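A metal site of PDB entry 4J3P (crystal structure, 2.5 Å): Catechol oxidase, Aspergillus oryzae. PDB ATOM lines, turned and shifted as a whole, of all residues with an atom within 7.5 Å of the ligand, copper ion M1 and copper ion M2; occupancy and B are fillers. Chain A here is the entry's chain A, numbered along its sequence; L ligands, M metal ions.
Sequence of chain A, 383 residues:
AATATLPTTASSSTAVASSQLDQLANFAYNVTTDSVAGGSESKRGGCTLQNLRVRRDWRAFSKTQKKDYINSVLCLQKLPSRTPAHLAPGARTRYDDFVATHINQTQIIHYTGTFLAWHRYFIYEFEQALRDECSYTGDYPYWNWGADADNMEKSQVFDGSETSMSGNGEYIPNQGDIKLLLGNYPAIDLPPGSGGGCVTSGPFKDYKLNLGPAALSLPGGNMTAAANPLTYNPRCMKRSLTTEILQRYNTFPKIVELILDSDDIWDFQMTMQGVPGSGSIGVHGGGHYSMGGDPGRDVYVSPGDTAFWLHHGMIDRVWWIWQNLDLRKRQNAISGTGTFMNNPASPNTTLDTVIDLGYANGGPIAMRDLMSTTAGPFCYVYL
Copper ion M1 is bound by a ring nitrogen (NE2) of His 102, an oxygen (O2) of the ligand, a ring nitrogen (NE2) of His 119 and a ring nitrogen (NE2) of His 110.
Copper ion M1 has four donor atoms within binding distance.
Phe 308 touches copper ion M2.
CE2 of Phe 308 touches O2 of the ligand (3.7 Å).
Hydrophobic or aromatic side chains within 4 Å of the ligand: His 102, His 110, His 119, His 288, Phe 308 and His 312.
An oxygen (O1) of the ligand sits close to the side-chain hydroxyl of Ser 302, 3.4 Å away.
The backbone carbonyl oxygen (O) of His 102 sits at hydrogen-bond distance from the side-chain hydroxyl (OG1) of Thr 106, at 2.8 Å.
The backbone carbonyl oxygen of Tyr 300 sits at hydrogen-bond distance from a ring nitrogen (ND1) of His 102 (2.9 Å).
A ring nitrogen (ND1) of His 119 sits at hydrogen-bond distance from the backbone carbonyl oxygen of Phe 115, at 2.9 Å.
A ring nitrogen (NE2) of His 311 lies within hydrogen-bond range of the backbone carbonyl oxygen of His 284 (3.1 Å).
O of Thr 106 lies within hydrogen-bond range of ND1 of His 110 (3.2 Å).
NE2 of His 288 binds copper ion M2 (1.9 Å).
NE2 of His 312 is bound to copper ion M2 (2.0 Å).
Copper ion M2 is bound by NE2 of His 284, 2.1 Å away.
Copper ion M2 is bound by O2 of the ligand, at 2.3 Å.
Within 4 Å of copper ion M1: His 102, His 110 and His 119.
Along chain A the residues within 4 Å of copper ion M1 span positions 102 to 119.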
ATOM      1  N   HIS A 102     -14.648  -5.013 -31.651  1.00  0.00           N
ATOM      2  CA  HIS A 102     -14.220  -4.307 -30.457  1.00  0.00           C
ATOM      3  C   HIS A 102     -15.257  -3.277 -30.027  1.00  0.00           C
ATOM      4  O   HIS A 102     -15.581  -3.178 -28.842  1.00  0.00           O
ATOM      5  CB  HIS A 102     -12.881  -3.624 -30.671  1.00  0.00           C
ATOM      6  CG  HIS A 102     -12.248  -3.149 -29.404  1.00  0.00           C
ATOM      7  ND1 HIS A 102     -12.538  -1.919 -28.850  1.00  0.00           N
ATOM      8  CD2 HIS A 102     -11.369  -3.741 -28.570  1.00  0.00           C
ATOM      9  CE1 HIS A 102     -11.854  -1.779 -27.727  1.00  0.00           C
ATOM     10  NE2 HIS A 102     -11.126  -2.867 -27.535  1.00  0.00           N
ATOM     11  N   GLN A 105     -18.296  -4.965 -28.457  1.00  0.00           N
ATOM     12  CA  GLN A 105     -18.197  -5.638 -27.177  1.00  0.00           C
ATOM     13  C   GLN A 105     -17.538  -4.799 -26.085  1.00  0.00           C
ATOM     14  O   GLN A 105     -17.212  -5.319 -25.025  1.00  0.00           O
ATOM     15  CB  GLN A 105     -17.439  -6.961 -27.331  1.00  0.00           C
ATOM     16  CG  GLN A 105     -18.032  -7.910 -28.358  1.00  0.00           C
ATOM     17  CD  GLN A 105     -17.386  -9.271 -28.332  1.00  0.00           C
ATOM     18  OE1 GLN A 105     -17.422  -9.955 -27.318  1.00  0.00           O
ATOM     19  NE2 GLN A 105     -16.775  -9.666 -29.438  1.00  0.00           N
ATOM     20  N   THR A 106     -17.325  -3.514 -26.362  1.00  0.00           N
ATOM     21  CA  THR A 106     -16.603  -2.628 -25.427  1.00  0.00           C
ATOM     22  C   THR A 106     -17.132  -2.711 -24.002  1.00  0.00           C
ATOM     23  O   THR A 106     -16.353  -2.726 -23.046  1.00  0.00           O
ATOM     24  CB  THR A 106     -16.624  -1.149 -25.939  1.00  0.00           C
ATOM     25  OG1 THR A 106     -15.685  -1.018 -27.015  1.00  0.00           O
ATOM     26  CG2 THR A 106     -16.240  -0.153 -24.839  1.00  0.00           C
ATOM     27  N   ILE A 109     -15.779  -5.892 -22.146  1.00  0.00           N
ATOM     28  CA  ILE A 109     -14.367  -6.256 -22.251  1.00  0.00           C
ATOM     29  C   ILE A 109     -13.413  -5.274 -21.585  1.00  0.00           C
ATOM     30  O   ILE A 109     -12.205  -5.448 -21.629  1.00  0.00           O
ATOM     31  CB  ILE A 109     -13.896  -6.465 -23.711  1.00  0.00           C
ATOM     32  CG1 ILE A 109     -13.980  -5.145 -24.485  1.00  0.00           C
ATOM     33  CG2 ILE A 109     -14.693  -7.586 -24.385  1.00  0.00           C
ATOM     34  CD1 ILE A 109     -13.709  -5.289 -25.978  1.00  0.00           C
ATOM     35  N   HIS A 110     -13.963  -4.233 -20.962  1.00  0.00           N
ATOM     36  CA  HIS A 110     -13.106  -3.340 -20.195  1.00  0.00           C
ATOM     37  C   HIS A 110     -13.642  -3.277 -18.795  1.00  0.00           C
ATOM     38  O   HIS A 110     -14.853  -3.342 -18.602  1.00  0.00           O
ATOM     39  CB  HIS A 110     -13.007  -1.972 -20.872  1.00  0.00           C
ATOM     40  CG  HIS A 110     -12.450  -2.034 -22.259  1.00  0.00           C
ATOM     41  ND1 HIS A 110     -13.244  -2.094 -23.376  1.00  0.00           N
ATOM     42  CD2 HIS A 110     -11.165  -2.090 -22.703  1.00  0.00           C
ATOM     43  CE1 HIS A 110     -12.477  -2.171 -24.460  1.00  0.00           C
ATOM     44  NE2 HIS A 110     -11.219  -2.175 -24.070  1.00  0.00           N
ATOM     45  N   PHE A 115     -11.132  -8.747 -19.206  1.00  0.00           N
ATOM     46  CA  PHE A 115     -10.345  -7.717 -19.870  1.00  0.00           C
ATOM     47  C   PHE A 115      -9.036  -8.220 -20.456  1.00  0.00           C
ATOM     48  O   PHE A 115      -8.799  -8.138 -21.664  1.00  0.00           O
ATOM     49  CB  PHE A 115     -10.062  -6.570 -18.913  1.00  0.00           C
ATOM     50  CG  PHE A 115      -9.003  -5.635 -19.402  1.00  0.00           C
ATOM     51  CD1 PHE A 115      -9.209  -4.878 -20.551  1.00  0.00           C
ATOM     52  CD2 PHE A 115      -7.805  -5.503 -18.731  1.00  0.00           C
ATOM     53  CE1 PHE A 115      -8.241  -4.015 -21.005  1.00  0.00           C
ATOM     54  CE2 PHE A 115      -6.831  -4.627 -19.188  1.00  0.00           C
ATOM     55  CZ  PHE A 115      -7.044  -3.881 -20.325  1.00  0.00           C
ATOM     56  N   TRP A 118      -9.319 -11.421 -22.916  1.00  0.00           N
ATOM     57  CA  TRP A 118     -10.038 -11.162 -24.158  1.00  0.00           C
ATOM     58  C   TRP A 118      -9.063 -10.465 -25.112  1.00  0.00           C
ATOM     59  O   TRP A 118      -8.930 -10.830 -26.283  1.00  0.00           O
ATOM     60  CB  TRP A 118     -11.292 -10.294 -23.898  1.00  0.00           C
ATOM     61  CG  TRP A 118     -12.129 -10.014 -25.130  1.00  0.00           C
ATOM     62  CD1 TRP A 118     -13.285 -10.629 -25.518  1.00  0.00           C
ATOM     63  CD2 TRP A 118     -11.851  -9.030 -26.148  1.00  0.00           C
ATOM     64  NE1 TRP A 118     -13.752 -10.101 -26.692  1.00  0.00           N
ATOM     65  CE2 TRP A 118     -12.880  -9.119 -27.105  1.00  0.00           C
ATOM     66  CE3 TRP A 118     -10.834  -8.104 -26.340  1.00  0.00           C
ATOM     67  CZ2 TRP A 118     -12.924  -8.312 -28.232  1.00  0.00           C
ATOM     68  CZ3 TRP A 118     -10.881  -7.292 -27.448  1.00  0.00           C
ATOM     69  CH2 TRP A 118     -11.909  -7.410 -28.388  1.00  0.00           C
ATOM     70  N   HIS A 119      -8.348  -9.469 -24.597  1.00  0.00           N
ATOM     71  CA  HIS A 119      -7.400  -8.746 -25.426  1.00  0.00           C
ATOM     72  C   HIS A 119      -6.254  -9.620 -25.898  1.00  0.00           C
ATOM     73  O   HIS A 119      -5.821  -9.519 -27.051  1.00  0.00           O
ATOM     74  CB  HIS A 119      -6.905  -7.484 -24.725  1.00  0.00           C
ATOM     75  CG  HIS A 119      -7.912  -6.374 -24.754  1.00  0.00           C
ATOM     76  ND1 HIS A 119      -9.013  -6.355 -23.933  1.00  0.00           N
ATOM     77  CD2 HIS A 119      -7.998  -5.274 -25.550  1.00  0.00           C
ATOM     78  CE1 HIS A 119      -9.726  -5.270 -24.194  1.00  0.00           C
ATOM     79  NE2 HIS A 119      -9.131  -4.600 -25.165  1.00  0.00           N
ATOM     80  N   PHE A 122      -7.690 -11.419 -28.642  1.00  0.00           N
ATOM     81  CA  PHE A 122      -7.948 -10.448 -29.713  1.00  0.00           C
ATOM     82  C   PHE A 122      -6.704 -10.214 -30.562  1.00  0.00           C
ATOM     83  O   PHE A 122      -6.756 -10.293 -31.795  1.00  0.00           O
ATOM     84  CB  PHE A 122      -8.450  -9.134 -29.106  1.00  0.00           C
ATOM     85  CG  PHE A 122      -9.001  -8.173 -30.102  1.00  0.00           C
ATOM     86  CD1 PHE A 122      -9.935  -8.564 -31.038  1.00  0.00           C
ATOM     87  CD2 PHE A 122      -8.601  -6.847 -30.083  1.00  0.00           C
ATOM     88  CE1 PHE A 122     -10.452  -7.667 -31.953  1.00  0.00           C
ATOM     89  CE2 PHE A 122      -9.113  -5.934 -30.991  1.00  0.00           C
ATOM     90  CZ  PHE A 122     -10.038  -6.345 -31.931  1.00  0.00           C
ATOM     91  N   HIS A 284      -2.290   1.533 -19.245  1.00  0.00           N
ATOM     92  CA  HIS A 284      -3.229   1.221 -20.325  1.00  0.00           C
ATOM     93  C   HIS A 284      -3.959   2.428 -20.876  1.00  0.00           C
ATOM     94  O   HIS A 284      -4.096   2.569 -22.079  1.00  0.00           O
ATOM     95  CB  HIS A 284      -4.244   0.168 -19.916  1.00  0.00           C
ATOM     96  CG  HIS A 284      -5.259  -0.099 -20.965  1.00  0.00           C
ATOM     97  ND1 HIS A 284      -6.567   0.329 -20.869  1.00  0.00           N
ATOM     98  CD2 HIS A 284      -5.166  -0.724 -22.164  1.00  0.00           C
ATOM     99  CE1 HIS A 284      -7.232  -0.038 -21.948  1.00  0.00           C
ATOM    100  NE2 HIS A 284      -6.403  -0.671 -22.760  1.00  0.00           N
ATOM    101  N   GLY A 285      -4.466   3.292 -19.999  1.00  0.00           N
ATOM    102  CA  GLY A 285      -5.151   4.481 -20.446  1.00  0.00           C
ATOM    103  C   GLY A 285      -4.110   5.461 -20.948  1.00  0.00           C
ATOM    104  O   GLY A 285      -4.337   6.220 -21.904  1.00  0.00           O
ATOM    105  N   HIS A 288      -3.075   4.477 -24.676  1.00  0.00           N
ATOM    106  CA  HIS A 288      -4.142   4.879 -25.586  1.00  0.00           C
ATOM    107  C   HIS A 288      -4.211   6.410 -25.775  1.00  0.00           C
ATOM    108  O   HIS A 288      -4.109   6.900 -26.890  1.00  0.00           O
ATOM    109  CB  HIS A 288      -5.501   4.388 -25.068  1.00  0.00           C
ATOM    110  CG  HIS A 288      -5.740   2.934 -25.294  1.00  0.00           C
ATOM    111  ND1 HIS A 288      -5.906   2.387 -26.549  1.00  0.00           N
ATOM    112  CD2 HIS A 288      -5.876   1.913 -24.413  1.00  0.00           C
ATOM    113  CE1 HIS A 288      -6.118   1.088 -26.433  1.00  0.00           C
ATOM    114  NE2 HIS A 288      -6.107   0.774 -25.146  1.00  0.00           N
ATOM    115  N   ASP A 298     -11.037   7.275 -28.175  1.00  0.00           N
ATOM    116  CA  ASP A 298     -12.325   6.596 -28.172  1.00  0.00           C
ATOM    117  C   ASP A 298     -12.142   5.151 -27.696  1.00  0.00           C
ATOM    118  O   ASP A 298     -11.714   4.280 -28.448  1.00  0.00           O
ATOM    119  CB  ASP A 298     -12.952   6.633 -29.577  1.00  0.00           C
ATOM    120  CG  ASP A 298     -14.365   6.047 -29.614  1.00  0.00           C
ATOM    121  OD1 ASP A 298     -14.574   4.929 -29.116  1.00  0.00           O
ATOM    122  OD2 ASP A 298     -15.259   6.696 -30.194  1.00  0.00           O
ATOM    123  N   VAL A 299     -12.495   4.926 -26.430  1.00  0.00           N
ATOM    124  CA  VAL A 299     -12.423   3.624 -25.807  1.00  0.00           C
ATOM    125  C   VAL A 299     -13.056   2.493 -26.631  1.00  0.00           C
ATOM    126  O   VAL A 299     -12.605   1.355 -26.561  1.00  0.00           O
ATOM    127  CB  VAL A 299     -13.024   3.682 -24.373  1.00  0.00           C
ATOM    128  CG1 VAL A 299     -13.429   2.311 -23.885  1.00  0.00           C
ATOM    129  CG2 VAL A 299     -12.045   4.346 -23.411  1.00  0.00           C
ATOM    130  N   TYR A 300     -14.073   2.792 -27.428  1.00  0.00           N
ATOM    131  CA  TYR A 300     -14.724   1.778 -28.251  1.00  0.00           C
ATOM    132  C   TYR A 300     -13.963   1.484 -29.534  1.00  0.00           C
ATOM    133  O   TYR A 300     -13.888   0.336 -29.962  1.00  0.00           O
ATOM    134  CB  TYR A 300     -16.131   2.213 -28.679  1.00  0.00           C
ATOM    135  CG  TYR A 300     -17.166   2.405 -27.588  1.00  0.00           C
ATOM    136  CD1 TYR A 300     -18.305   1.601 -27.535  1.00  0.00           C
ATOM    137  CD2 TYR A 300     -17.038   3.405 -26.651  1.00  0.00           C
ATOM    138  CE1 TYR A 300     -19.278   1.786 -26.557  1.00  0.00           C
ATOM    139  CE2 TYR A 300     -17.980   3.595 -25.659  1.00  0.00           C
ATOM    140  CZ  TYR A 300     -19.103   2.782 -25.622  1.00  0.00           C
ATOM    141  OH  TYR A 300     -20.039   3.006 -24.638  1.00  0.00           O
ATOM    142  N   VAL A 301     -13.461   2.540 -30.163  1.00  0.00           N
ATOM    143  CA  VAL A 301     -12.962   2.435 -31.539  1.00  0.00           C
ATOM    144  C   VAL A 301     -11.431   2.348 -31.588  1.00  0.00           C
ATOM    145  O   VAL A 301     -10.843   2.256 -32.663  1.00  0.00           O
ATOM    146  CB  VAL A 301     -13.477   3.625 -32.376  1.00  0.00           C
ATOM    147  CG1 VAL A 301     -13.282   3.380 -33.877  1.00  0.00           C
ATOM    148  CG2 VAL A 301     -14.950   3.835 -32.099  1.00  0.00           C
ATOM    149  N   SER A 302     -10.807   2.319 -30.423  1.00  0.00           N
ATOM    150  CA  SER A 302      -9.342   2.345 -30.342  1.00  0.00           C
ATOM    151  C   SER A 302      -8.550   1.406 -31.264  1.00  0.00           C
ATOM    152  O   SER A 302      -7.453   1.761 -31.686  1.00  0.00           O
ATOM    153  CB  SER A 302      -8.884   2.192 -28.903  1.00  0.00           C
ATOM    154  OG  SER A 302      -9.453   1.045 -28.336  1.00  0.00           O
ATOM    155  N   PRO A 303      -9.069   0.210 -31.590  1.00  0.00           N
ATOM    156  CA  PRO A 303      -8.286  -0.604 -32.533  1.00  0.00           C
ATOM    157  C   PRO A 303      -8.181   0.009 -33.924  1.00  0.00           C
ATOM    158  O   PRO A 303      -7.381  -0.449 -34.749  1.00  0.00           O
ATOM    159  CB  PRO A 303      -9.077  -1.901 -32.626  1.00  0.00           C
ATOM    160  CG  PRO A 303      -9.870  -1.956 -31.421  1.00  0.00           C
ATOM    161  CD  PRO A 303     -10.205  -0.551 -31.049  1.00  0.00           C
ATOM    162  N   PHE A 308      -2.540   0.431 -31.694  1.00  0.00           N
ATOM    163  CA  PHE A 308      -3.275  -0.394 -30.748  1.00  0.00           C
ATOM    164  C   PHE A 308      -2.642  -1.768 -30.556  1.00  0.00           C
ATOM    165  O   PHE A 308      -2.482  -2.236 -29.429  1.00  0.00           O
ATOM    166  CB  PHE A 308      -4.714  -0.565 -31.248  1.00  0.00           C
ATOM    167  CG  PHE A 308      -5.548  -1.476 -30.421  1.00  0.00           C
ATOM    168  CD1 PHE A 308      -5.614  -2.845 -30.715  1.00  0.00           C
ATOM    169  CD2 PHE A 308      -6.297  -0.983 -29.358  1.00  0.00           C
ATOM    170  CE1 PHE A 308      -6.385  -3.694 -29.955  1.00  0.00           C
ATOM    171  CE2 PHE A 308      -7.079  -1.834 -28.590  1.00  0.00           C
ATOM    172  CZ  PHE A 308      -7.126  -3.194 -28.882  1.00  0.00           C
ATOM    173  N   HIS A 311       0.670  -1.499 -28.575  1.00  0.00           N
ATOM    174  CA  HIS A 311       0.243  -1.127 -27.230  1.00  0.00           C
ATOM    175  C   HIS A 311      -0.251  -2.367 -26.475  1.00  0.00           C
ATOM    176  O   HIS A 311       0.187  -2.669 -25.367  1.00  0.00           O
ATOM    177  CB  HIS A 311      -0.845  -0.052 -27.305  1.00  0.00           C
ATOM    178  CG  HIS A 311      -1.418   0.334 -25.974  1.00  0.00           C
ATOM    179  ND1 HIS A 311      -0.643   0.831 -24.951  1.00  0.00           N
ATOM    180  CD2 HIS A 311      -2.689   0.302 -25.507  1.00  0.00           C
ATOM    181  CE1 HIS A 311      -1.413   1.095 -23.910  1.00  0.00           C
ATOM    182  NE2 HIS A 311      -2.658   0.782 -24.215  1.00  0.00           N
ATOM    183  N   HIS A 312      -1.161  -3.102 -27.088  1.00  0.00           N
ATOM    184  CA  HIS A 312      -1.707  -4.263 -26.411  1.00  0.00           C
ATOM    185  C   HIS A 312      -0.774  -5.451 -26.426  1.00  0.00           C
ATOM    186  O   HIS A 312      -0.970  -6.397 -25.664  1.00  0.00           O
ATOM    187  CB  HIS A 312      -3.104  -4.609 -26.916  1.00  0.00           C
ATOM    188  CG  HIS A 312      -4.174  -3.864 -26.186  1.00  0.00           C
ATOM    189  ND1 HIS A 312      -4.778  -4.354 -25.050  1.00  0.00           N
ATOM    190  CD2 HIS A 312      -4.708  -2.645 -26.400  1.00  0.00           C
ATOM    191  CE1 HIS A 312      -5.664  -3.474 -24.615  1.00  0.00           C
ATOM    192  NE2 HIS A 312      -5.630  -2.425 -25.413  1.00  0.00           N
ATOM    193  N   ILE A 315       0.767  -4.635 -23.210  1.00  0.00           N
ATOM    194  CA  ILE A 315      -0.170  -4.900 -22.133  1.00  0.00           C
ATOM    195  C   ILE A 315      -0.130  -6.377 -21.795  1.00  0.00           C
ATOM    196  O   ILE A 315      -0.026  -6.768 -20.632  1.00  0.00           O
ATOM    197  CB  ILE A 315      -1.618  -4.548 -22.558  1.00  0.00           C
ATOM    198  CG1 ILE A 315      -1.788  -3.037 -22.747  1.00  0.00           C
ATOM    199  CG2 ILE A 315      -2.615  -5.101 -21.537  1.00  0.00           C
ATOM    200  CD1 ILE A 315      -1.707  -2.243 -21.447  1.00  0.00           C
HETATM  201  O1  LIG L   1      -9.297  -0.679 -25.363  1.00  0.00           O
HETATM  202  O2  LIG L   1      -8.835  -1.785 -25.351  1.00  0.00           O
HETATM  203 CU    CU M   1     -10.311  -3.072 -25.784  1.00  0.00          CU
HETATM  204 CU    CU M   2      -6.795  -0.937 -24.807  1.00  0.00          CU
